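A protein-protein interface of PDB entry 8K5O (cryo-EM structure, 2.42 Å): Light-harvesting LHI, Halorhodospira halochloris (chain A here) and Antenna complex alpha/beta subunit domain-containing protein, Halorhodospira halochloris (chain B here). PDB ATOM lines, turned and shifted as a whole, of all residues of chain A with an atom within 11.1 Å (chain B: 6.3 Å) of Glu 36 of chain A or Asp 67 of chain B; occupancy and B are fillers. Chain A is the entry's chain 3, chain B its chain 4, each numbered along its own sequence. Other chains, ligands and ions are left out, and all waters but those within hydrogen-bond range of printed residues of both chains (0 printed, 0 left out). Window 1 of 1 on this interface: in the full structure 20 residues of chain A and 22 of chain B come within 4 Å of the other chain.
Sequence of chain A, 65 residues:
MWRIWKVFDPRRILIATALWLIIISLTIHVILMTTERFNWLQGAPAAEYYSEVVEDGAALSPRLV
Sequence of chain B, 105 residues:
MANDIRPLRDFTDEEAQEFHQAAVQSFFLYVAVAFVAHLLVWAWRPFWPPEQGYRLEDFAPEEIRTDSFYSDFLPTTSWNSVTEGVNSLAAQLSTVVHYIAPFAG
OE1 of Glu 36 of chain A lies close to O of Asp 67 of chain B, at 2.8 Å.
NH2 of Arg 45 of chain B is in hydrogen-bond range of O of Ala 44 of chain A, at 2.5 Å.
N of Ala 46 of chain A lies close to NH2 of Arg 45 of chain B (3.0 Å).
O of Arg 37 of chain A sits close to NH1 of Arg 45 of chain B.
OE2 of Glu 57 of chain B is in salt-bridge range of NE of Arg 55 of chain B (3.2 Å).
The backbone carbonyl oxygen (O) of Leu 32 of chain A sits at hydrogen-bond distance from the side-chain hydroxyl (OG1) of Thr 35 of chain A (2.4 Å).
OD1 of Asn 39 of chain A is in hydrogen-bond range of N of Gln 42 of chain A (3.3 Å).
The guanidinium group of Arg 37 of chain A lies within salt-bridge range of the side-chain carboxylate of Glu 48 of chain A, at 2.4 Å.
The backbone NH (N) of Phe 38 of chain A is in hydrogen-bond range of the side-chain hydroxyl (OG1) of Thr 35 of chain A, at 3.3 Å.
Thr 34 of chain A touches Phe 69 of chain B.
Thr 35 of chain A touches Phe 69 of chain B.
Glu 36 of chain A touches Arg 65 of chain B.
Thr 66 of chain B touches Glu 36 of chain A.
NE2 of Gln 42 of chain A touches NH2 of Arg 65 of chain B, at 3.98 Å.
Pro 45 of chain A touches Arg 45 of chain B (C to NH2, 3.2 Å).
O of Pro 45 of chain A touches CD1 of Leu 56 of chain B, 3.4 Å away.
CD1 of Leu 56 of chain B touches O of Ala 46 of chain A, 3.5 Å away.
Arg 55 of chain B touches Ala 47 of chain A (O to CB, 3.9 Å).
Ala 47 of chain A touches Leu 56 of chain B.
Of chain B, only Leu 56, Arg 65, Thr 66 and Asp 67 come within 4 Å of Glu 36 of chain A.
Asp 67 of chain B touches one residue of chain A.
Arg 65 of chain B touches two residues of chain A.
No residue of chain A comes within 4 Å of Ser 68 of chain B.
Of the printed residues of chain B, Thr 34 of chain A touches Phe 69.
Of the printed residues of chain B, Arg 37 of chain A touches Arg 45 (2.4 Å).
Printed residues of chain B within 4 Å of Ala 46 of chain A: Arg 45 (3.0 Å) and Leu 56 (3.5 Å).
Printed residues of chain A within 4 Å of Arg 45 of chain B: Arg 37 (2.4 Å), Phe 38 (3.5 Å), Ala 44 (2.5 Å), Pro 45 (3.2 Å) and Ala 46 (3.0 Å).
Printed residues of chain B within 4 Å of Ala 47 of chain A: Arg 55 (3.9 Å) and Leu 56 (3.7 Å).
Val 30 of chain A touches none of the printed residues of chain B.
Of the 11 printed residues of chain B, 8 touch a printed residue of chain A.
Hydrophobic or aromatic side chains of chain B within 4 Å of the printed part of chain A: Leu 56, Ile 64 and Phe 69.
Hydrophobic or aromatic side chains of chain A within 4 Å of the printed part of chain B: Phe 38, Pro 45, Ala 46 and Ala 47.
Along chain A the printed residues that touch a printed residue of chain B span positions 34 to 51.
Among the printed residues, no Asp or Glu carboxylate lies within 4 Å of a Lys or Arg side-chain nitrogen of the other chain.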
ATOM      1  N   ILE A  28      -5.072   4.509  20.237  1.00  0.00           N
ATOM      2  CA  ILE A  28      -5.980   3.492  19.732  1.00  0.00           C
ATOM      3  C   ILE A  28      -6.529   2.650  20.868  1.00  0.00           C
ATOM      4  O   ILE A  28      -7.717   2.321  20.887  1.00  0.00           O
ATOM      5  CB  ILE A  28      -5.290   2.605  18.685  1.00  0.00           C
ATOM      6  CG1 ILE A  28      -4.916   3.405  17.448  1.00  0.00           C
ATOM      7  CG2 ILE A  28      -6.203   1.483  18.310  1.00  0.00           C
ATOM      8  CD1 ILE A  28      -3.727   2.840  16.747  1.00  0.00           C
ATOM      9  N   HIS A  29      -5.675   2.259  21.816  1.00  0.00           N
ATOM     10  CA  HIS A  29      -6.161   1.464  22.935  1.00  0.00           C
ATOM     11  C   HIS A  29      -7.238   2.214  23.711  1.00  0.00           C
ATOM     12  O   HIS A  29      -8.287   1.647  24.040  1.00  0.00           O
ATOM     13  CB  HIS A  29      -4.996   1.070  23.842  1.00  0.00           C
ATOM     14  CG  HIS A  29      -4.188  -0.081  23.325  1.00  0.00           C
ATOM     15  ND1 HIS A  29      -3.037   0.083  22.588  1.00  0.00           N
ATOM     16  CD2 HIS A  29      -4.363  -1.417  23.450  1.00  0.00           C
ATOM     17  CE1 HIS A  29      -2.537  -1.100  22.282  1.00  0.00           C
ATOM     18  NE2 HIS A  29      -3.322  -2.029  22.796  1.00  0.00           N
ATOM     19  N   VAL A  30      -7.020   3.507  23.967  1.00  0.00           N
ATOM     20  CA  VAL A  30      -8.013   4.293  24.694  1.00  0.00           C
ATOM     21  C   VAL A  30      -9.276   4.476  23.857  1.00  0.00           C
ATOM     22  O   VAL A  30     -10.395   4.463  24.385  1.00  0.00           O
ATOM     23  CB  VAL A  30      -7.411   5.643  25.129  1.00  0.00           C
ATOM     24  CG1 VAL A  30      -8.445   6.467  25.864  1.00  0.00           C
ATOM     25  CG2 VAL A  30      -6.200   5.424  26.013  1.00  0.00           C
ATOM     26  N   ILE A  31      -9.121   4.639  22.543  1.00  0.00           N
ATOM     27  CA  ILE A  31     -10.274   4.776  21.661  1.00  0.00           C
ATOM     28  C   ILE A  31     -11.123   3.513  21.699  1.00  0.00           C
ATOM     29  O   ILE A  31     -12.357   3.577  21.737  1.00  0.00           O
ATOM     30  CB  ILE A  31      -9.811   5.114  20.231  1.00  0.00           C
ATOM     31  CG1 ILE A  31      -9.473   6.597  20.115  1.00  0.00           C
ATOM     32  CG2 ILE A  31     -10.872   4.746  19.216  1.00  0.00           C
ATOM     33  CD1 ILE A  31      -8.633   6.930  18.912  1.00  0.00           C
ATOM     34  N   LEU A  32     -10.476   2.348  21.682  1.00  0.00           N
ATOM     35  CA  LEU A  32     -11.201   1.089  21.822  1.00  0.00           C
ATOM     36  C   LEU A  32     -11.888   1.006  23.173  1.00  0.00           C
ATOM     37  O   LEU A  32     -12.999   0.476  23.282  1.00  0.00           O
ATOM     38  CB  LEU A  32     -10.253  -0.091  21.646  1.00  0.00           C
ATOM     39  CG  LEU A  32      -9.485  -0.148  20.333  1.00  0.00           C
ATOM     40  CD1 LEU A  32      -8.790  -1.481  20.208  1.00  0.00           C
ATOM     41  CD2 LEU A  32     -10.420   0.111  19.166  1.00  0.00           C
ATOM     42  N   MET A  33     -11.231   1.506  24.217  1.00  0.00           N
ATOM     43  CA  MET A  33     -11.868   1.570  25.526  1.00  0.00           C
ATOM     44  C   MET A  33     -13.132   2.421  25.484  1.00  0.00           C
ATOM     45  O   MET A  33     -14.102   2.136  26.195  1.00  0.00           O
ATOM     46  CB  MET A  33     -10.886   2.117  26.554  1.00  0.00           C
ATOM     47  CG  MET A  33      -9.716   1.209  26.815  1.00  0.00           C
ATOM     48  SD  MET A  33      -8.466   2.020  27.814  1.00  0.00           S
ATOM     49  CE  MET A  33      -7.183   0.779  27.817  1.00  0.00           C
ATOM     50  N   THR A  34     -13.139   3.475  24.663  1.00  0.00           N
ATOM     51  CA  THR A  34     -14.346   4.284  24.523  1.00  0.00           C
ATOM     52  C   THR A  34     -15.444   3.568  23.751  1.00  0.00           C
ATOM     53  O   THR A  34     -16.603   3.986  23.821  1.00  0.00           O
ATOM     54  CB  THR A  34     -14.044   5.615  23.832  1.00  0.00           C
ATOM     55  OG1 THR A  34     -13.373   5.374  22.590  1.00  0.00           O
ATOM     56  CG2 THR A  34     -13.187   6.495  24.714  1.00  0.00           C
ATOM     57  N   THR A  35     -15.114   2.519  23.009  1.00  0.00           N
ATOM     58  CA  THR A  35     -16.129   1.811  22.250  1.00  0.00           C
ATOM     59  C   THR A  35     -16.875   0.828  23.144  1.00  0.00           C
ATOM     60  O   THR A  35     -16.507   0.577  24.292  1.00  0.00           O
ATOM     61  CB  THR A  35     -15.511   1.080  21.058  1.00  0.00           C
ATOM     62  OG1 THR A  35     -14.644   0.041  21.523  1.00  0.00           O
ATOM     63  CG2 THR A  35     -14.726   2.042  20.193  1.00  0.00           C
ATOM     64  N   GLU A  36     -17.958   0.282  22.604  1.00  0.00           N
ATOM     65  CA  GLU A  36     -18.719  -0.757  23.276  1.00  0.00           C
ATOM     66  C   GLU A  36     -18.320  -2.147  22.817  1.00  0.00           C
ATOM     67  O   GLU A  36     -18.206  -3.060  23.638  1.00  0.00           O
ATOM     68  CB  GLU A  36     -20.214  -0.554  23.032  1.00  0.00           C
ATOM     69  CG  GLU A  36     -21.091  -1.539  23.764  1.00  0.00           C
ATOM     70  CD  GLU A  36     -22.553  -1.352  23.455  1.00  0.00           C
ATOM     71  OE1 GLU A  36     -22.869  -0.494  22.608  1.00  0.00           O
ATOM     72  OE2 GLU A  36     -23.384  -2.067  24.049  1.00  0.00           O
ATOM     73  N   ARG A  37     -18.084  -2.321  21.519  1.00  0.00           N
ATOM     74  CA  ARG A  37     -17.781  -3.649  21.009  1.00  0.00           C
ATOM     75  C   ARG A  37     -16.364  -4.064  21.366  1.00  0.00           C
ATOM     76  O   ARG A  37     -16.109  -5.233  21.671  1.00  0.00           O
ATOM     77  CB  ARG A  37     -17.959  -3.679  19.499  1.00  0.00           C
ATOM     78  CG  ARG A  37     -17.641  -5.011  18.873  1.00  0.00           C
ATOM     79  CD  ARG A  37     -17.678  -4.827  17.409  1.00  0.00           C
ATOM     80  NE  ARG A  37     -17.372  -5.977  16.575  1.00  0.00           N
ATOM     81  CZ  ARG A  37     -18.237  -6.938  16.289  1.00  0.00           C
ATOM     82  NH1 ARG A  37     -19.464  -6.934  16.780  1.00  0.00           N
ATOM     83  NH2 ARG A  37     -17.869  -7.915  15.470  1.00  0.00           N
ATOM     84  N   PHE A  38     -15.430  -3.122  21.326  1.00  0.00           N
ATOM     85  CA  PHE A  38     -14.014  -3.426  21.441  1.00  0.00           C
ATOM     86  C   PHE A  38     -13.437  -3.085  22.803  1.00  0.00           C
ATOM     87  O   PHE A  38     -12.222  -3.172  22.981  1.00  0.00           O
ATOM     88  CB  PHE A  38     -13.240  -2.693  20.352  1.00  0.00           C
ATOM     89  CG  PHE A  38     -13.780  -2.919  18.982  1.00  0.00           C
ATOM     90  CD1 PHE A  38     -13.783  -4.185  18.428  1.00  0.00           C
ATOM     91  CD2 PHE A  38     -14.284  -1.870  18.245  1.00  0.00           C
ATOM     92  CE1 PHE A  38     -14.261  -4.392  17.160  1.00  0.00           C
ATOM     93  CE2 PHE A  38     -14.769  -2.078  16.981  1.00  0.00           C
ATOM     94  CZ  PHE A  38     -14.758  -3.340  16.440  1.00  0.00           C
ATOM     95  N   ASN A  39     -14.268  -2.695  23.766  1.00  0.00           N
ATOM     96  CA  ASN A  39     -13.796  -2.458  25.126  1.00  0.00           C
ATOM     97  C   ASN A  39     -13.759  -3.804  25.835  1.00  0.00           C
ATOM     98  O   ASN A  39     -14.754  -4.276  26.383  1.00  0.00           O
ATOM     99  CB  ASN A  39     -14.680  -1.456  25.853  1.00  0.00           C
ATOM    100  CG  ASN A  39     -14.010  -0.874  27.076  1.00  0.00           C
ATOM    101  OD1 ASN A  39     -12.940  -1.316  27.480  1.00  0.00           O
ATOM    102  ND2 ASN A  39     -14.637   0.128  27.670  1.00  0.00           N
ATOM    103  N   TRP A  40     -12.588  -4.436  25.799  1.00  0.00           N
ATOM    104  CA  TRP A  40     -12.375  -5.685  26.516  1.00  0.00           C
ATOM    105  C   TRP A  40     -12.483  -5.492  28.022  1.00  0.00           C
ATOM    106  O   TRP A  40     -12.820  -6.436  28.744  1.00  0.00           O
ATOM    107  CB  TRP A  40     -11.012  -6.264  26.133  1.00  0.00           C
ATOM    108  CG  TRP A  40      -9.845  -5.409  26.552  1.00  0.00           C
ATOM    109  CD1 TRP A  40      -8.967  -5.666  27.560  1.00  0.00           C
ATOM    110  CD2 TRP A  40      -9.438  -4.159  25.977  1.00  0.00           C
ATOM    111  NE1 TRP A  40      -8.039  -4.660  27.646  1.00  0.00           N
ATOM    112  CE2 TRP A  40      -8.306  -3.723  26.686  1.00  0.00           C
ATOM    113  CE3 TRP A  40      -9.917  -3.370  24.927  1.00  0.00           C
ATOM    114  CZ2 TRP A  40      -7.650  -2.531  26.385  1.00  0.00           C
ATOM    115  CZ3 TRP A  40      -9.264  -2.190  24.629  1.00  0.00           C
ATOM    116  CH2 TRP A  40      -8.142  -1.785  25.352  1.00  0.00           C
ATOM    117  N   LEU A  41     -12.195  -4.285  28.511  1.00  0.00           N
ATOM    118  CA  LEU A  41     -12.316  -4.007  29.936  1.00  0.00           C
ATOM    119  C   LEU A  41     -13.777  -3.975  30.367  1.00  0.00           C
ATOM    120  O   LEU A  41     -14.147  -4.567  31.387  1.00  0.00           O
ATOM    121  CB  LEU A  41     -11.624  -2.685  30.261  1.00  0.00           C
ATOM    122  CG  LEU A  41     -10.157  -2.587  29.838  1.00  0.00           C
ATOM    123  CD1 LEU A  41      -9.649  -1.170  30.003  1.00  0.00           C
ATOM    124  CD2 LEU A  41      -9.307  -3.559  30.631  1.00  0.00           C
ATOM    125  N   GLN A  42     -14.620  -3.281  29.601  1.00  0.00           N
ATOM    126  CA  GLN A  42     -16.048  -3.252  29.895  1.00  0.00           C
ATOM    127  C   GLN A  42     -16.704  -4.592  29.580  1.00  0.00           C
ATOM    128  O   GLN A  42     -17.637  -5.011  30.273  1.00  0.00           O
ATOM    129  CB  GLN A  42     -16.714  -2.123  29.111  1.00  0.00           C
ATOM    130  CG  GLN A  42     -18.207  -1.995  29.338  1.00  0.00           C
ATOM    131  CD  GLN A  42     -18.953  -1.569  28.091  1.00  0.00           C
ATOM    132  OE1 GLN A  42     -18.352  -1.126  27.112  1.00  0.00           O
ATOM    133  NE2 GLN A  42     -20.272  -1.716  28.114  1.00  0.00           N
ATOM    134  N   GLY A  43     -16.230  -5.276  28.547  1.00  0.00           N
ATOM    135  CA  GLY A  43     -16.722  -6.601  28.212  1.00  0.00           C
ATOM    136  C   GLY A  43     -18.144  -6.677  27.698  1.00  0.00           C
ATOM    137  O   GLY A  43     -18.867  -7.621  28.035  1.00  0.00           O
ATOM    138  N   ALA A  44     -18.555  -5.725  26.868  1.00  0.00           N
ATOM    139  CA  ALA A  44     -19.910  -5.733  26.343  1.00  0.00           C
ATOM    140  C   ALA A  44     -20.081  -6.842  25.305  1.00  0.00           C
ATOM    141  O   ALA A  44     -19.114  -7.253  24.661  1.00  0.00           O
ATOM    142  CB  ALA A  44     -20.248  -4.381  25.725  1.00  0.00           C
ATOM    143  N   PRO A  45     -21.300  -7.344  25.129  1.00  0.00           N
ATOM    144  CA  PRO A  45     -21.535  -8.382  24.122  1.00  0.00           C
ATOM    145  C   PRO A  45     -21.351  -7.855  22.709  1.00  0.00           C
ATOM    146  O   PRO A  45     -21.434  -6.656  22.436  1.00  0.00           O
ATOM    147  CB  PRO A  45     -22.990  -8.797  24.360  1.00  0.00           C
ATOM    148  CG  PRO A  45     -23.357  -8.235  25.681  1.00  0.00           C
ATOM    149  CD  PRO A  45     -22.519  -7.030  25.887  1.00  0.00           C
ATOM    150  N   ALA A  46     -21.083  -8.784  21.802  1.00  0.00           N
ATOM    151  CA  ALA A  46     -20.979  -8.470  20.389  1.00  0.00           C
ATOM    152  C   ALA A  46     -22.330  -8.640  19.708  1.00  0.00           C
ATOM    153  O   ALA A  46     -23.162  -9.455  20.112  1.00  0.00           O
ATOM    154  CB  ALA A  46     -19.935  -9.355  19.712  1.00  0.00           C
ATOM    155  N   ALA A  47     -22.539  -7.854  18.652  1.00  0.00           N
ATOM    156  CA  ALA A  47     -23.790  -7.917  17.910  1.00  0.00           C
ATOM    157  C   ALA A  47     -23.982  -9.249  17.201  1.00  0.00           C
ATOM    158  O   ALA A  47     -25.123  -9.614  16.906  1.00  0.00           O
ATOM    159  CB  ALA A  47     -23.852  -6.778  16.897  1.00  0.00           C
ATOM    160  N   GLU A  48     -22.901  -9.979  16.915  1.00  0.00           N
ATOM    161  CA  GLU A  48     -23.037 -11.284  16.279  1.00  0.00           C
ATOM    162  C   GLU A  48     -23.748 -12.277  17.185  1.00  0.00           C
ATOM    163  O   GLU A  48     -24.370 -13.229  16.701  1.00  0.00           O
ATOM    164  CB  GLU A  48     -21.662 -11.823  15.891  1.00  0.00           C
ATOM    165  CG  GLU A  48     -21.031 -11.130  14.704  1.00  0.00           C
ATOM    166  CD  GLU A  48     -20.191  -9.938  15.108  1.00  0.00           C
ATOM    167  OE1 GLU A  48     -20.574  -9.233  16.062  1.00  0.00           O
ATOM    168  OE2 GLU A  48     -19.145  -9.705  14.469  1.00  0.00           O
ATOM    169  N   TYR A  50     -26.266 -11.455  19.221  1.00  0.00           N
ATOM    170  CA  TYR A  50     -27.640 -11.005  19.452  1.00  0.00           C
ATOM    171  C   TYR A  50     -28.002 -11.144  20.932  1.00  0.00           C
ATOM    172  O   TYR A  50     -28.953 -11.831  21.308  1.00  0.00           O
ATOM    173  CB  TYR A  50     -28.631 -11.766  18.564  1.00  0.00           C
ATOM    174  CG  TYR A  50     -28.111 -12.082  17.185  1.00  0.00           C
ATOM    175  CD1 TYR A  50     -27.674 -11.076  16.341  1.00  0.00           C
ATOM    176  CD2 TYR A  50     -28.051 -13.391  16.727  1.00  0.00           C
ATOM    177  CE1 TYR A  50     -27.192 -11.359  15.081  1.00  0.00           C
ATOM    178  CE2 TYR A  50     -27.572 -13.684  15.466  1.00  0.00           C
ATOM    179  CZ  TYR A  50     -27.143 -12.663  14.649  1.00  0.00           C
ATOM    180  OH  TYR A  50     -26.666 -12.942  13.392  1.00  0.00           O
ATOM    181  N   SER A  51     -27.215 -10.468  21.765  1.00  0.00           N
ATOM    182  CA  SER A  51     -27.228 -10.654  23.217  1.00  0.00           C
ATOM    183  C   SER A  51     -28.612 -10.722  23.840  1.00  0.00           C
ATOM    184  O   SER A  51     -28.769 -11.206  24.959  1.00  0.00           O
ATOM    185  CB  SER A  51     -26.440  -9.534  23.889  1.00  0.00           C
ATOM    186  OG  SER A  51     -26.193  -9.844  25.249  1.00  0.00           O
ATOM    187  N   ARG B  45     -13.499 -10.005  17.261  1.00  0.00           N
ATOM    188  CA  ARG B  45     -14.595  -9.149  16.837  1.00  0.00           C
ATOM    189  C   ARG B  45     -14.173  -8.349  15.614  1.00  0.00           C
ATOM    190  O   ARG B  45     -13.304  -7.475  15.718  1.00  0.00           O
ATOM    191  CB  ARG B  45     -15.026  -8.218  17.969  1.00  0.00           C
ATOM    192  CG  ARG B  45     -15.749  -8.937  19.073  1.00  0.00           C
ATOM    193  CD  ARG B  45     -16.262  -8.010  20.117  1.00  0.00           C
ATOM    194  NE  ARG B  45     -17.010  -8.751  21.118  1.00  0.00           N
ATOM    195  CZ  ARG B  45     -17.679  -8.196  22.113  1.00  0.00           C
ATOM    196  NH1 ARG B  45     -17.748  -6.885  22.249  1.00  0.00           N
ATOM    197  NH2 ARG B  45     -18.319  -8.976  22.976  1.00  0.00           N
ATOM    198  N   ARG B  55     -23.879  -2.536  15.640  1.00  0.00           N
ATOM    199  CA  ARG B  55     -24.313  -1.902  16.873  1.00  0.00           C
ATOM    200  C   ARG B  55     -25.101  -2.910  17.697  1.00  0.00           C
ATOM    201  O   ARG B  55     -26.019  -3.557  17.188  1.00  0.00           O
ATOM    202  CB  ARG B  55     -25.162  -0.680  16.562  1.00  0.00           C
ATOM    203  CG  ARG B  55     -24.363   0.540  16.212  1.00  0.00           C
ATOM    204  CD  ARG B  55     -25.231   1.770  16.256  1.00  0.00           C
ATOM    205  NE  ARG B  55     -26.497   1.543  15.571  1.00  0.00           N
ATOM    206  CZ  ARG B  55     -27.348   2.501  15.240  1.00  0.00           C
ATOM    207  NH1 ARG B  55     -27.087   3.772  15.489  1.00  0.00           N
ATOM    208  NH2 ARG B  55     -28.486   2.177  14.635  1.00  0.00           N
ATOM    209  N   LEU B  56     -24.736  -3.049  18.972  1.00  0.00           N
ATOM    210  CA  LEU B  56     -25.392  -4.036  19.822  1.00  0.00           C
ATOM    211  C   LEU B  56     -26.876  -3.738  19.989  1.00  0.00           C
ATOM    212  O   LEU B  56     -27.682  -4.663  20.123  1.00  0.00           O
ATOM    213  CB  LEU B  56     -24.697  -4.093  21.182  1.00  0.00           C
ATOM    214  CG  LEU B  56     -25.056  -5.276  22.081  1.00  0.00           C
ATOM    215  CD1 LEU B  56     -24.665  -6.597  21.446  1.00  0.00           C
ATOM    216  CD2 LEU B  56     -24.413  -5.117  23.441  1.00  0.00           C
ATOM    217  N   GLU B  57     -27.253  -2.460  19.972  1.00  0.00           N
ATOM    218  CA  GLU B  57     -28.658  -2.089  20.093  1.00  0.00           C
ATOM    219  C   GLU B  57     -29.487  -2.597  18.922  1.00  0.00           C
ATOM    220  O   GLU B  57     -30.703  -2.766  19.053  1.00  0.00           O
ATOM    221  CB  GLU B  57     -28.772  -0.572  20.212  1.00  0.00           C
ATOM    222  CG  GLU B  57     -28.253   0.176  19.001  1.00  0.00           C
ATOM    223  CD  GLU B  57     -28.303   1.672  19.188  1.00  0.00           C
ATOM    224  OE1 GLU B  57     -28.733   2.123  20.268  1.00  0.00           O
ATOM    225  OE2 GLU B  57     -27.916   2.403  18.256  1.00  0.00           O
ATOM    226  N   ILE B  64     -30.782  -6.059  27.253  1.00  0.00           N
ATOM    227  CA  ILE B  64     -29.334  -5.915  27.185  1.00  0.00           C
ATOM    228  C   ILE B  64     -29.021  -4.430  27.100  1.00  0.00           C
ATOM    229  O   ILE B  64     -29.500  -3.737  26.196  1.00  0.00           O
ATOM    230  CB  ILE B  64     -28.751  -6.675  25.985  1.00  0.00           C
ATOM    231  CG1 ILE B  64     -29.111  -8.157  26.073  1.00  0.00           C
ATOM    232  CG2 ILE B  64     -27.246  -6.492  25.918  1.00  0.00           C
ATOM    233  CD1 ILE B  64     -28.563  -8.848  27.300  1.00  0.00           C
ATOM    234  N   ARG B  65     -28.226  -3.938  28.046  1.00  0.00           N
ATOM    235  CA  ARG B  65     -27.875  -2.524  28.091  1.00  0.00           C
ATOM    236  C   ARG B  65     -26.854  -2.233  27.002  1.00  0.00           C
ATOM    237  O   ARG B  65     -25.732  -2.745  27.037  1.00  0.00           O
ATOM    238  CB  ARG B  65     -27.327  -2.146  29.462  1.00  0.00           C
ATOM    239  CG  ARG B  65     -26.966  -0.681  29.581  1.00  0.00           C
ATOM    240  CD  ARG B  65     -26.395  -0.365  30.945  1.00  0.00           C
ATOM    241  NE  ARG B  65     -25.166  -1.103  31.205  1.00  0.00           N
ATOM    242  CZ  ARG B  65     -23.967  -0.742  30.770  1.00  0.00           C
ATOM    243  NH1 ARG B  65     -23.796   0.347  30.041  1.00  0.00           N
ATOM    244  NH2 ARG B  65     -22.914  -1.494  31.076  1.00  0.00           N
ATOM    245  N   THR B  66     -27.242  -1.408  26.037  1.00  0.00           N
ATOM    246  CA  THR B  66     -26.362  -0.964  24.970  1.00  0.00           C
ATOM    247  C   THR B  66     -26.145   0.533  25.115  1.00  0.00           C
ATOM    248  O   THR B  66     -27.109   1.294  25.232  1.00  0.00           O
ATOM    249  CB  THR B  66     -26.952  -1.284  23.595  1.00  0.00           C
ATOM    250  OG1 THR B  66     -28.057  -0.411  23.336  1.00  0.00           O
ATOM    251  CG2 THR B  66     -27.424  -2.726  23.535  1.00  0.00           C
ATOM    252  N   ASP B  67     -24.885   0.948  25.118  1.00  0.00           N
ATOM    253  CA  ASP B  67     -24.522   2.349  25.252  1.00  0.00           C
ATOM    254  C   ASP B  67     -23.911   2.820  23.941  1.00  0.00           C
ATOM    255  O   ASP B  67     -22.972   2.201  23.434  1.00  0.00           O
ATOM    256  CB  ASP B  67     -23.538   2.549  26.408  1.00  0.00           C
ATOM    257  CG  ASP B  67     -23.393   4.002  26.809  1.00  0.00           C
ATOM    258  OD1 ASP B  67     -24.053   4.864  26.193  1.00  0.00           O
ATOM    259  OD2 ASP B  67     -22.611   4.282  27.743  1.00  0.00           O
ATOM    260  N   SER B  68     -24.451   3.903  23.394  1.00  0.00           N
ATOM    261  CA  SER B  68     -23.957   4.423  22.128  1.00  0.00           C
ATOM    262  C   SER B  68     -22.537   4.951  22.277  1.00  0.00           C
ATOM    263  O   SER B  68     -22.120   5.388  23.353  1.00  0.00           O
ATOM    264  CB  SER B  68     -24.874   5.528  21.615  1.00  0.00           C
ATOM    265  OG  SER B  68     -24.843   6.649  22.478  1.00  0.00           O
ATOM    266  N   PHE B  69     -21.785   4.898  21.175  1.00  0.00           N
ATOM    267  CA  PHE B  69     -20.438   5.453  21.178  1.00  0.00           C
ATOM    268  C   PHE B  69     -20.466   6.945  21.469  1.00  0.00           C
ATOM    269  O   PHE B  69     -19.643   7.451  22.240  1.00  0.00           O
ATOM    270  CB  PHE B  69     -19.757   5.180  19.835  1.00  0.00           C
ATOM    271  CG  PHE B  69     -18.401   5.804  19.702  1.00  0.00           C
ATOM    272  CD1 PHE B  69     -17.275   5.150  20.167  1.00  0.00           C
ATOM    273  CD2 PHE B  69     -18.251   7.039  19.097  1.00  0.00           C
ATOM    274  CE1 PHE B  69     -16.028   5.723  20.043  1.00  0.00           C
ATOM    275  CE2 PHE B  69     -17.011   7.614  18.975  1.00  0.00           C
ATOM    276  CZ  PHE B  69     -15.897   6.956  19.444  1.00  0.00           C
ATOM    277  N   TYR B  70     -21.438   7.633  20.919  1.00  0.00           N
ATOM    278  CA  TYR B  70     -21.522   9.027  21.138  1.00  0.00           C
ATOM    279  C   TYR B  70     -22.198   9.320  22.440  1.00  0.00           C
ATOM    280  O   TYR B  70     -23.199   8.720  22.754  1.00  0.00           O
ATOM    281  CB  TYR B  70     -22.256   9.691  19.979  1.00  0.00           C
ATOM    282  CG  TYR B  70     -21.669   9.456  18.633  1.00  0.00           C
ATOM    283  CD1 TYR B  70     -20.353   9.778  18.361  1.00  0.00           C
ATOM    284  CD2 TYR B  70     -22.437   8.929  17.630  1.00  0.00           C
ATOM    285  CE1 TYR B  70     -19.821   9.570  17.117  1.00  0.00           C
ATOM    286  CE2 TYR B  70     -21.916   8.707  16.387  1.00  0.00           C
ATOM    287  CZ  TYR B  70     -20.616   9.032  16.136  1.00  0.00           C
ATOM    288  OH  TYR B  70     -20.142   8.798  14.893  1.00  0.00           O
